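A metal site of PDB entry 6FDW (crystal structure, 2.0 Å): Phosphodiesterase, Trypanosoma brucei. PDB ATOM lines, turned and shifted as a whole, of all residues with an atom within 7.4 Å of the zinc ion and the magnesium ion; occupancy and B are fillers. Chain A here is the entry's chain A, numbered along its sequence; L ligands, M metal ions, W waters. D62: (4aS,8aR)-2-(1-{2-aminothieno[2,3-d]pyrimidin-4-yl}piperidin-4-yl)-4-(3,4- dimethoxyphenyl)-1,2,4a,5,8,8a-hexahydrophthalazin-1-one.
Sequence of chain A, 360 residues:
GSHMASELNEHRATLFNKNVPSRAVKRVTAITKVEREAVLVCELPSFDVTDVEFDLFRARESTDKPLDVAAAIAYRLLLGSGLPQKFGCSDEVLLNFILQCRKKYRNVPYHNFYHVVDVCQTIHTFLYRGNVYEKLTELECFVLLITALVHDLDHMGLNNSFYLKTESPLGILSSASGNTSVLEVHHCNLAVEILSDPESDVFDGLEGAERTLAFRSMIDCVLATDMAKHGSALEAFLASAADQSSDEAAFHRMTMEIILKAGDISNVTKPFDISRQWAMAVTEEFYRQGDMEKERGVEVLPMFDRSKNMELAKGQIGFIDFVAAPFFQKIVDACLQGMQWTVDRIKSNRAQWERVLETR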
ATOM      1  N   TYR A 110      19.681 -33.663 -11.864  1.00  0.00           N
ATOM      2  CA  TYR A 110      19.600 -32.184 -11.587  1.00  0.00           C
ATOM      3  C   TYR A 110      19.512 -31.354 -12.878  1.00  0.00           C
ATOM      4  O   TYR A 110      18.545 -30.656 -13.078  1.00  0.00           O
ATOM      5  CB  TYR A 110      20.785 -31.702 -10.736  1.00  0.00           C
ATOM      6  CG  TYR A 110      20.691 -30.236 -10.353  1.00  0.00           C
ATOM      7  CD1 TYR A 110      19.814 -29.808  -9.330  1.00  0.00           C
ATOM      8  CD2 TYR A 110      21.351 -29.279 -11.058  1.00  0.00           C
ATOM      9  CE1 TYR A 110      19.663 -28.462  -9.006  1.00  0.00           C
ATOM     10  CE2 TYR A 110      21.223 -27.911 -10.732  1.00  0.00           C
ATOM     11  CZ  TYR A 110      20.385 -27.499  -9.679  1.00  0.00           C
ATOM     12  OH  TYR A 110      20.255 -26.167  -9.343  1.00  0.00           O
ATOM     13  N   HIS A 111      20.542 -31.438 -13.718  1.00  0.00           N
ATOM     14  CA  HIS A 111      20.614 -30.665 -14.944  1.00  0.00           C
ATOM     15  C   HIS A 111      19.781 -31.149 -16.077  1.00  0.00           C
ATOM     16  O   HIS A 111      20.244 -31.422 -17.122  1.00  0.00           O
ATOM     17  CB  HIS A 111      22.036 -30.520 -15.410  1.00  0.00           C
ATOM     18  CG  HIS A 111      22.858 -29.682 -14.515  1.00  0.00           C
ATOM     19  ND1 HIS A 111      23.779 -30.204 -13.660  1.00  0.00           N
ATOM     20  CD2 HIS A 111      22.893 -28.353 -14.333  1.00  0.00           C
ATOM     21  CE1 HIS A 111      24.358 -29.229 -13.001  1.00  0.00           C
ATOM     22  NE2 HIS A 111      23.840 -28.095 -13.384  1.00  0.00           N
ATOM     23  N   HIS A 115      15.291 -28.008 -14.067  1.00  0.00           N
ATOM     24  CA  HIS A 115      16.274 -26.993 -13.634  1.00  0.00           C
ATOM     25  C   HIS A 115      16.109 -25.742 -14.484  1.00  0.00           C
ATOM     26  O   HIS A 115      15.961 -24.666 -13.925  1.00  0.00           O
ATOM     27  CB  HIS A 115      17.715 -27.525 -13.730  1.00  0.00           C
ATOM     28  CG  HIS A 115      18.765 -26.459 -13.627  1.00  0.00           C
ATOM     29  ND1 HIS A 115      18.993 -25.748 -12.462  1.00  0.00           N
ATOM     30  CD2 HIS A 115      19.654 -26.009 -14.533  1.00  0.00           C
ATOM     31  CE1 HIS A 115      19.964 -24.888 -12.677  1.00  0.00           C
ATOM     32  NE2 HIS A 115      20.354 -24.986 -13.929  1.00  0.00           N
ATOM     33  N   VAL A 116      15.978 -25.881 -15.819  1.00  0.00           N
ATOM     34  CA  VAL A 116      16.048 -24.644 -16.682  1.00  0.00           C
ATOM     35  C   VAL A 116      14.746 -23.927 -16.674  1.00  0.00           C
ATOM     36  O   VAL A 116      14.695 -22.722 -16.685  1.00  0.00           O
ATOM     37  CB  VAL A 116      16.644 -24.888 -18.132  1.00  0.00           C
ATOM     38  CG1 VAL A 116      18.035 -25.499 -18.040  1.00  0.00           C
ATOM     39  CG2 VAL A 116      15.777 -25.734 -19.041  1.00  0.00           C
ATOM     40  N   VAL A 119      14.913 -22.034 -13.500  1.00  0.00           N
ATOM     41  CA  VAL A 119      15.779 -20.821 -13.674  1.00  0.00           C
ATOM     42  C   VAL A 119      15.057 -19.718 -14.376  1.00  0.00           C
ATOM     43  O   VAL A 119      15.020 -18.565 -13.871  1.00  0.00           O
ATOM     44  CB  VAL A 119      17.132 -21.121 -14.342  1.00  0.00           C
ATOM     45  CG1 VAL A 119      17.921 -19.853 -14.633  1.00  0.00           C
ATOM     46  CG2 VAL A 119      17.953 -22.028 -13.438  1.00  0.00           C
ATOM     47  N   ALA A 148      17.506 -18.446 -20.139  1.00  0.00           N
ATOM     48  CA  ALA A 148      17.306 -19.421 -19.057  1.00  0.00           C
ATOM     49  C   ALA A 148      17.088 -20.847 -19.637  1.00  0.00           C
ATOM     50  O   ALA A 148      17.682 -21.844 -19.163  1.00  0.00           O
ATOM     51  CB  ALA A 148      16.130 -18.957 -18.192  1.00  0.00           C
ATOM     52  N   HIS A 151      20.382 -22.543 -21.268  1.00  0.00           N
ATOM     53  CA  HIS A 151      21.708 -22.316 -20.647  1.00  0.00           C
ATOM     54  C   HIS A 151      22.489 -23.550 -20.214  1.00  0.00           C
ATOM     55  O   HIS A 151      23.709 -23.445 -19.908  1.00  0.00           O
ATOM     56  CB  HIS A 151      21.594 -21.305 -19.441  1.00  0.00           C
ATOM     57  CG  HIS A 151      21.269 -21.967 -18.124  1.00  0.00           C
ATOM     58  ND1 HIS A 151      19.983 -22.160 -17.736  1.00  0.00           N
ATOM     59  CD2 HIS A 151      22.055 -22.466 -17.125  1.00  0.00           C
ATOM     60  CE1 HIS A 151      19.967 -22.781 -16.559  1.00  0.00           C
ATOM     61  NE2 HIS A 151      21.212 -22.995 -16.179  1.00  0.00           N
ATOM     62  N   ASP A 152      21.836 -24.710 -20.261  1.00  0.00           N
ATOM     63  CA  ASP A 152      22.461 -25.977 -19.923  1.00  0.00           C
ATOM     64  C   ASP A 152      21.988 -27.056 -20.884  1.00  0.00           C
ATOM     65  O   ASP A 152      21.706 -28.189 -20.478  1.00  0.00           O
ATOM     66  CB  ASP A 152      22.126 -26.366 -18.485  1.00  0.00           C
ATOM     67  CG  ASP A 152      22.956 -25.615 -17.459  1.00  0.00           C
ATOM     68  OD1 ASP A 152      24.168 -25.420 -17.702  1.00  0.00           O
ATOM     69  OD2 ASP A 152      22.398 -25.218 -16.418  1.00  0.00           O
ATOM     70  N   LEU A 153      21.882 -26.732 -22.161  1.00  0.00           N
ATOM     71  CA  LEU A 153      21.412 -27.676 -23.166  1.00  0.00           C
ATOM     72  C   LEU A 153      22.350 -28.834 -23.322  1.00  0.00           C
ATOM     73  O   LEU A 153      23.499 -28.624 -23.407  1.00  0.00           O
ATOM     74  CB  LEU A 153      21.266 -27.012 -24.519  1.00  0.00           C
ATOM     75  CG  LEU A 153      20.090 -26.099 -24.744  1.00  0.00           C
ATOM     76  CD1 LEU A 153      20.395 -25.221 -25.923  1.00  0.00           C
ATOM     77  CD2 LEU A 153      18.825 -26.863 -24.940  1.00  0.00           C
ATOM     78  N   HIS A 155      23.215 -31.138 -21.137  1.00  0.00           N
ATOM     79  CA  HIS A 155      24.047 -31.389 -19.993  1.00  0.00           C
ATOM     80  C   HIS A 155      24.001 -32.880 -19.678  1.00  0.00           C
ATOM     81  O   HIS A 155      22.987 -33.474 -19.799  1.00  0.00           O
ATOM     82  CB  HIS A 155      23.559 -30.585 -18.794  1.00  0.00           C
ATOM     83  CG  HIS A 155      24.600 -30.375 -17.752  1.00  0.00           C
ATOM     84  ND1 HIS A 155      25.103 -31.390 -16.995  1.00  0.00           N
ATOM     85  CD2 HIS A 155      25.219 -29.260 -17.325  1.00  0.00           C
ATOM     86  CE1 HIS A 155      26.006 -30.920 -16.162  1.00  0.00           C
ATOM     87  NE2 HIS A 155      26.086 -29.627 -16.344  1.00  0.00           N
ATOM     88  N   LEU A 183      31.428 -27.012 -20.974  1.00  0.00           N
ATOM     89  CA  LEU A 183      29.984 -27.227 -21.266  1.00  0.00           C
ATOM     90  C   LEU A 183      29.274 -25.961 -21.769  1.00  0.00           C
ATOM     91  O   LEU A 183      28.395 -25.987 -22.616  1.00  0.00           O
ATOM     92  CB  LEU A 183      29.235 -27.679 -20.037  1.00  0.00           C
ATOM     93  CG  LEU A 183      29.633 -29.056 -19.502  1.00  0.00           C
ATOM     94  CD1 LEU A 183      29.076 -29.279 -18.092  1.00  0.00           C
ATOM     95  CD2 LEU A 183      29.178 -30.129 -20.487  1.00  0.00           C
ATOM     96  N   GLU A 184      29.705 -24.822 -21.283  1.00  0.00           N
ATOM     97  CA  GLU A 184      28.982 -23.595 -21.613  1.00  0.00           C
ATOM     98  C   GLU A 184      29.110 -23.277 -23.104  1.00  0.00           C
ATOM     99  O   GLU A 184      28.120 -22.900 -23.734  1.00  0.00           O
ATOM    100  CB  GLU A 184      29.526 -22.451 -20.764  1.00  0.00           C
ATOM    101  CG  GLU A 184      29.152 -22.570 -19.285  1.00  0.00           C
ATOM    102  CD  GLU A 184      29.880 -23.668 -18.507  1.00  0.00           C
ATOM    103  OE1 GLU A 184      30.971 -24.121 -18.953  1.00  0.00           O
ATOM    104  OE2 GLU A 184      29.358 -24.064 -17.438  1.00  0.00           O
ATOM    105  N   HIS A 187      26.728 -25.534 -24.758  1.00  0.00           N
ATOM    106  CA  HIS A 187      25.329 -25.083 -24.664  1.00  0.00           C
ATOM    107  C   HIS A 187      25.093 -23.924 -25.678  1.00  0.00           C
ATOM    108  O   HIS A 187      24.065 -23.784 -26.290  1.00  0.00           O
ATOM    109  CB  HIS A 187      24.993 -24.581 -23.198  1.00  0.00           C
ATOM    110  CG  HIS A 187      25.340 -25.561 -22.118  1.00  0.00           C
ATOM    111  ND1 HIS A 187      25.018 -26.895 -22.218  1.00  0.00           N
ATOM    112  CD2 HIS A 187      26.007 -25.421 -20.952  1.00  0.00           C
ATOM    113  CE1 HIS A 187      25.468 -27.535 -21.148  1.00  0.00           C
ATOM    114  NE2 HIS A 187      26.094 -26.665 -20.383  1.00  0.00           N
ATOM    115  N   VAL A 222      25.275 -17.189 -20.915  1.00  0.00           N
ATOM    116  CA  VAL A 222      25.549 -18.646 -20.733  1.00  0.00           C
ATOM    117  C   VAL A 222      27.025 -18.867 -20.448  1.00  0.00           C
ATOM    118  O   VAL A 222      27.370 -19.662 -19.587  1.00  0.00           O
ATOM    119  CB  VAL A 222      25.190 -19.442 -21.982  1.00  0.00           C
ATOM    120  CG1 VAL A 222      25.647 -20.886 -21.857  1.00  0.00           C
ATOM    121  CG2 VAL A 222      23.719 -19.359 -22.291  1.00  0.00           C
ATOM    122  N   THR A 225      27.903 -18.432 -16.736  1.00  0.00           N
ATOM    123  CA  THR A 225      27.458 -19.434 -15.771  1.00  0.00           C
ATOM    124  C   THR A 225      28.487 -20.445 -15.341  1.00  0.00           C
ATOM    125  O   THR A 225      28.239 -21.236 -14.404  1.00  0.00           O
ATOM    126  CB  THR A 225      26.234 -20.205 -16.224  1.00  0.00           C
ATOM    127  OG1 THR A 225      26.537 -21.043 -17.372  1.00  0.00           O
ATOM    128  CG2 THR A 225      25.085 -19.243 -16.536  1.00  0.00           C
ATOM    129  N   ASP A 226      29.641 -20.459 -16.003  1.00  0.00           N
ATOM    130  CA  ASP A 226      30.750 -21.293 -15.524  1.00  0.00           C
ATOM    131  C   ASP A 226      31.203 -20.844 -14.138  1.00  0.00           C
ATOM    132  O   ASP A 226      31.750 -19.738 -13.988  1.00  0.00           O
ATOM    133  CB  ASP A 226      31.915 -21.225 -16.516  1.00  0.00           C
ATOM    134  CG  ASP A 226      33.103 -22.165 -16.130  1.00  0.00           C
ATOM    135  OD1 ASP A 226      33.159 -22.732 -15.016  1.00  0.00           O
ATOM    136  OD2 ASP A 226      34.025 -22.261 -16.961  1.00  0.00           O
ATOM    137  N   MET A 227      31.017 -21.708 -13.131  1.00  0.00           N
ATOM    138  CA  MET A 227      31.343 -21.344 -11.723  1.00  0.00           C
ATOM    139  C   MET A 227      32.834 -21.072 -11.444  1.00  0.00           C
ATOM    140  O   MET A 227      33.161 -20.473 -10.402  1.00  0.00           O
ATOM    141  CB  MET A 227      30.733 -22.324 -10.693  1.00  0.00           C
ATOM    142  CG  MET A 227      29.172 -22.254 -10.505  1.00  0.00           C
ATOM    143  SD  MET A 227      28.536 -20.611 -10.013  1.00  0.00           S
ATOM    144  CE  MET A 227      29.142 -20.566  -8.318  1.00  0.00           C
ATOM    145  N   LEU A 260      21.246 -14.088 -14.558  1.00  0.00           N
ATOM    146  CA  LEU A 260      21.217 -15.542 -14.942  1.00  0.00           C
ATOM    147  C   LEU A 260      22.003 -16.333 -13.940  1.00  0.00           C
ATOM    148  O   LEU A 260      21.522 -17.366 -13.534  1.00  0.00           O
ATOM    149  CB  LEU A 260      21.809 -15.820 -16.328  1.00  0.00           C
ATOM    150  CG  LEU A 260      21.820 -17.284 -16.778  1.00  0.00           C
ATOM    151  CD1 LEU A 260      20.415 -17.879 -16.846  1.00  0.00           C
ATOM    152  CD2 LEU A 260      22.488 -17.454 -18.102  1.00  0.00           C
ATOM    153  N   GLY A 263      19.810 -16.840 -10.883  1.00  0.00           N
ATOM    154  CA  GLY A 263      18.837 -17.905 -11.034  1.00  0.00           C
ATOM    155  C   GLY A 263      19.491 -19.263 -10.903  1.00  0.00           C
ATOM    156  O   GLY A 263      18.942 -20.188 -10.319  1.00  0.00           O
ATOM    157  N   ASP A 264      20.676 -19.385 -11.467  1.00  0.00           N
ATOM    158  CA  ASP A 264      21.401 -20.648 -11.428  1.00  0.00           C
ATOM    159  C   ASP A 264      21.714 -21.124 -10.029  1.00  0.00           C
ATOM    160  O   ASP A 264      21.737 -22.311  -9.802  1.00  0.00           O
ATOM    161  CB  ASP A 264      22.731 -20.516 -12.156  1.00  0.00           C
ATOM    162  CG  ASP A 264      23.034 -21.687 -13.089  1.00  0.00           C
ATOM    163  OD1 ASP A 264      22.223 -22.611 -13.177  1.00  0.00           O
ATOM    164  OD2 ASP A 264      24.128 -21.712 -13.645  1.00  0.00           O
ATOM    165  N   ILE A 265      22.006 -20.192  -9.107  1.00  0.00           N
ATOM    166  CA  ILE A 265      22.300 -20.565  -7.704  1.00  0.00           C
ATOM    167  C   ILE A 265      21.150 -20.146  -6.742  1.00  0.00           C
ATOM    168  O   ILE A 265      21.375 -19.953  -5.539  1.00  0.00           O
ATOM    169  CB  ILE A 265      23.673 -20.002  -7.210  1.00  0.00           C
ATOM    170  CG1 ILE A 265      23.747 -18.494  -7.280  1.00  0.00           C
ATOM    171  CG2 ILE A 265      24.877 -20.645  -7.955  1.00  0.00           C
ATOM    172  CD1 ILE A 265      25.038 -17.980  -6.655  1.00  0.00           C
HETATM  173  C1  D62 L   1      20.995 -27.299  -4.205  1.00  0.00           C
HETATM  174  N2  D62 L   1      28.379 -26.149  -8.459  1.00  0.00           N
HETATM  175  C3  D62 L   1      22.834 -26.557  -6.221  1.00  0.00           C
HETATM  176  C4  D62 L   1      23.764 -26.346  -7.212  1.00  0.00           C
HETATM  177  C5  D62 L   1      25.113 -26.489  -6.960  1.00  0.00           C
HETATM  178  C6  D62 L   1      26.155 -26.272  -8.006  1.00  0.00           C
HETATM  179  C12 D62 L   1      31.362 -24.798  -1.769  1.00  0.00           C
HETATM  180  C13 D62 L   1      29.895 -26.732  -1.481  1.00  0.00           C
HETATM  181  C14 D62 L   1      30.081 -26.461  -2.785  1.00  0.00           C
HETATM  182  C15 D62 L   1      31.010 -25.374  -2.971  1.00  0.00           C
HETATM  183  C16 D62 L   1      31.040 -24.323  -6.532  1.00  0.00           C
HETATM  184  C17 D62 L   1      29.750 -24.553  -7.238  1.00  0.00           C
HETATM  185  C18 D62 L   1      28.226 -25.972  -9.795  1.00  0.00           C
HETATM  186  C20 D62 L   1      26.616 -25.923 -11.822  1.00  0.00           C
HETATM  187  C21 D62 L   1      26.168 -24.501 -11.923  1.00  0.00           C
HETATM  188  C22 D62 L   1      25.690 -23.793 -10.918  1.00  0.00           C
HETATM  189  C23 D62 L   1      25.534 -24.329  -9.534  1.00  0.00           C
HETATM  190  C26 D62 L   1      24.602 -27.070  -4.645  1.00  0.00           C
HETATM  191  O1  D62 L   1      22.380 -27.119  -3.869  1.00  0.00           O
HETATM  192  C2  D62 L   1      23.232 -26.898  -4.926  1.00  0.00           C
HETATM  193  N1  D62 L   1      27.368 -26.412  -7.617  1.00  0.00           N
HETATM  194  C7  D62 L   1      29.683 -25.983  -7.756  1.00  0.00           C
HETATM  195  C8  D62 L   1      29.909 -26.986  -6.625  1.00  0.00           C
HETATM  196  C9  D62 L   1      31.143 -26.688  -5.811  1.00  0.00           C
HETATM  197  N3  D62 L   1      31.208 -25.267  -5.413  1.00  0.00           N
HETATM  198  C10 D62 L   1      31.530 -24.804  -4.145  1.00  0.00           C
HETATM  199  N4  D62 L   1      32.375 -23.743  -4.020  1.00  0.00           N
HETATM  200  C11 D62 L   1      32.674 -23.248  -2.790  1.00  0.00           C
HETATM  201  N5  D62 L   1      33.529 -22.186  -2.700  1.00  0.00           N
HETATM  202  N6  D62 L   1      32.190 -23.753  -1.635  1.00  0.00           N
HETATM  203  S1  D62 L   1      30.656 -25.586  -0.432  1.00  0.00           S
HETATM  204  O2  D62 L   1      29.135 -25.478 -10.456  1.00  0.00           O
HETATM  205  C19 D62 L   1      26.879 -26.371 -10.371  1.00  0.00           C
HETATM  206  C24 D62 L   1      25.761 -25.850  -9.426  1.00  0.00           C
HETATM  207  C25 D62 L   1      25.532 -26.851  -5.677  1.00  0.00           C
HETATM  208  O3  D62 L   1      24.898 -27.444  -3.360  1.00  0.00           O
HETATM  209  C27 D62 L   1      26.226 -27.859  -3.030  1.00  0.00           C
HETATM  210 ZN    ZN M   1      22.169 -24.294 -14.744  1.00  0.00          ZN
HETATM  211 MG    MG M   2      25.603 -24.742 -16.435  1.00  0.00          MG
HETATM  212  O   HOH W   1      25.721 -26.390 -14.972  1.00  0.00           O
HETATM  213  O   HOH W   2      23.285 -25.377 -13.198  1.00  0.00           O
HETATM  214  O   HOH W   3      23.991 -24.018 -15.125  1.00  0.00           O
HETATM  215  O   HOH W   4      25.664 -23.540 -17.682  1.00  0.00           O
HETATM  216  O   HOH W   5      27.248 -23.940 -15.741  1.00  0.00           O
HETATM  217  O   HOH W   6      26.732 -26.104 -17.511  1.00  0.00           O
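Water W4 lies within hydrogen-bond range of OG1 of Thr 225 and O of His 151.
Water W5 lies within hydrogen-bond range of the side-chain carboxylate (OE2) of Glu 184 (2.7 Å) and the backbone carbonyl oxygen (O) of Thr 225 (3.2 Å).
Water W6 lies within hydrogen-bond range of a ring nitrogen (NE2) of His 187 (3.0 Å) and the side-chain carboxylate (OE2) of Glu 184 (3.3 Å).
Water W3 binds the zinc ion (1.9 Å).
The side-chain carboxylate (OD2) of Asp 152 binds the zinc ion (1.9 Å).
The zinc ion is bound by NE2 of His 115, at 2.1 Å.
NE2 of His 151 binds the zinc ion, 2.2 Å away.
Water W2 binds the zinc ion, 2.2 Å away.
The zinc ion is bound by the side-chain carboxylate (OD1) of Asp 264, 2.3 Å away.
A ring nitrogen (ND1) of His 115 sits at hydrogen-bond distance from the side-chain hydroxyl of Tyr 110, 3.4 Å away.
A ring nitrogen (ND1) of His 151 sits at hydrogen-bond distance from the backbone carbonyl oxygen (O) of Ala 148 (2.7 Å).
The side-chain hydroxyl (OG1) of Thr 225 lies within hydrogen-bond range of the backbone carbonyl oxygen (O) of Val 222 (2.7 Å).
Four residues have an atom within 4 Å of the zinc ion: His 115, His 151, Asp 152 and Asp 264.
Along chain A the residues within 4 Å of the zinc ion span positions 115 to 264.
The nearest printed residue that does not touch the zinc ion is His 111 (4.1 Å).
The magnesium ion is bound by water W4 (1.7 Å), water W5 (2.0 Å), the side-chain carboxylate of Asp 152 (2.0 Å), water W6 (2.1 Å), water W3 (2.2 Å) and water W1 (2.2 Å).
The magnesium ion has six donor atoms within binding distance.
Glu 184 touches the magnesium ion (OE2 to MG, 3.9 Å).
OG1 of Thr 225 touches the magnesium ion, at 3.9 Å.
Three residues have an atom within 4 Å of the magnesium ion: Asp 152, Glu 184 and Thr 225.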
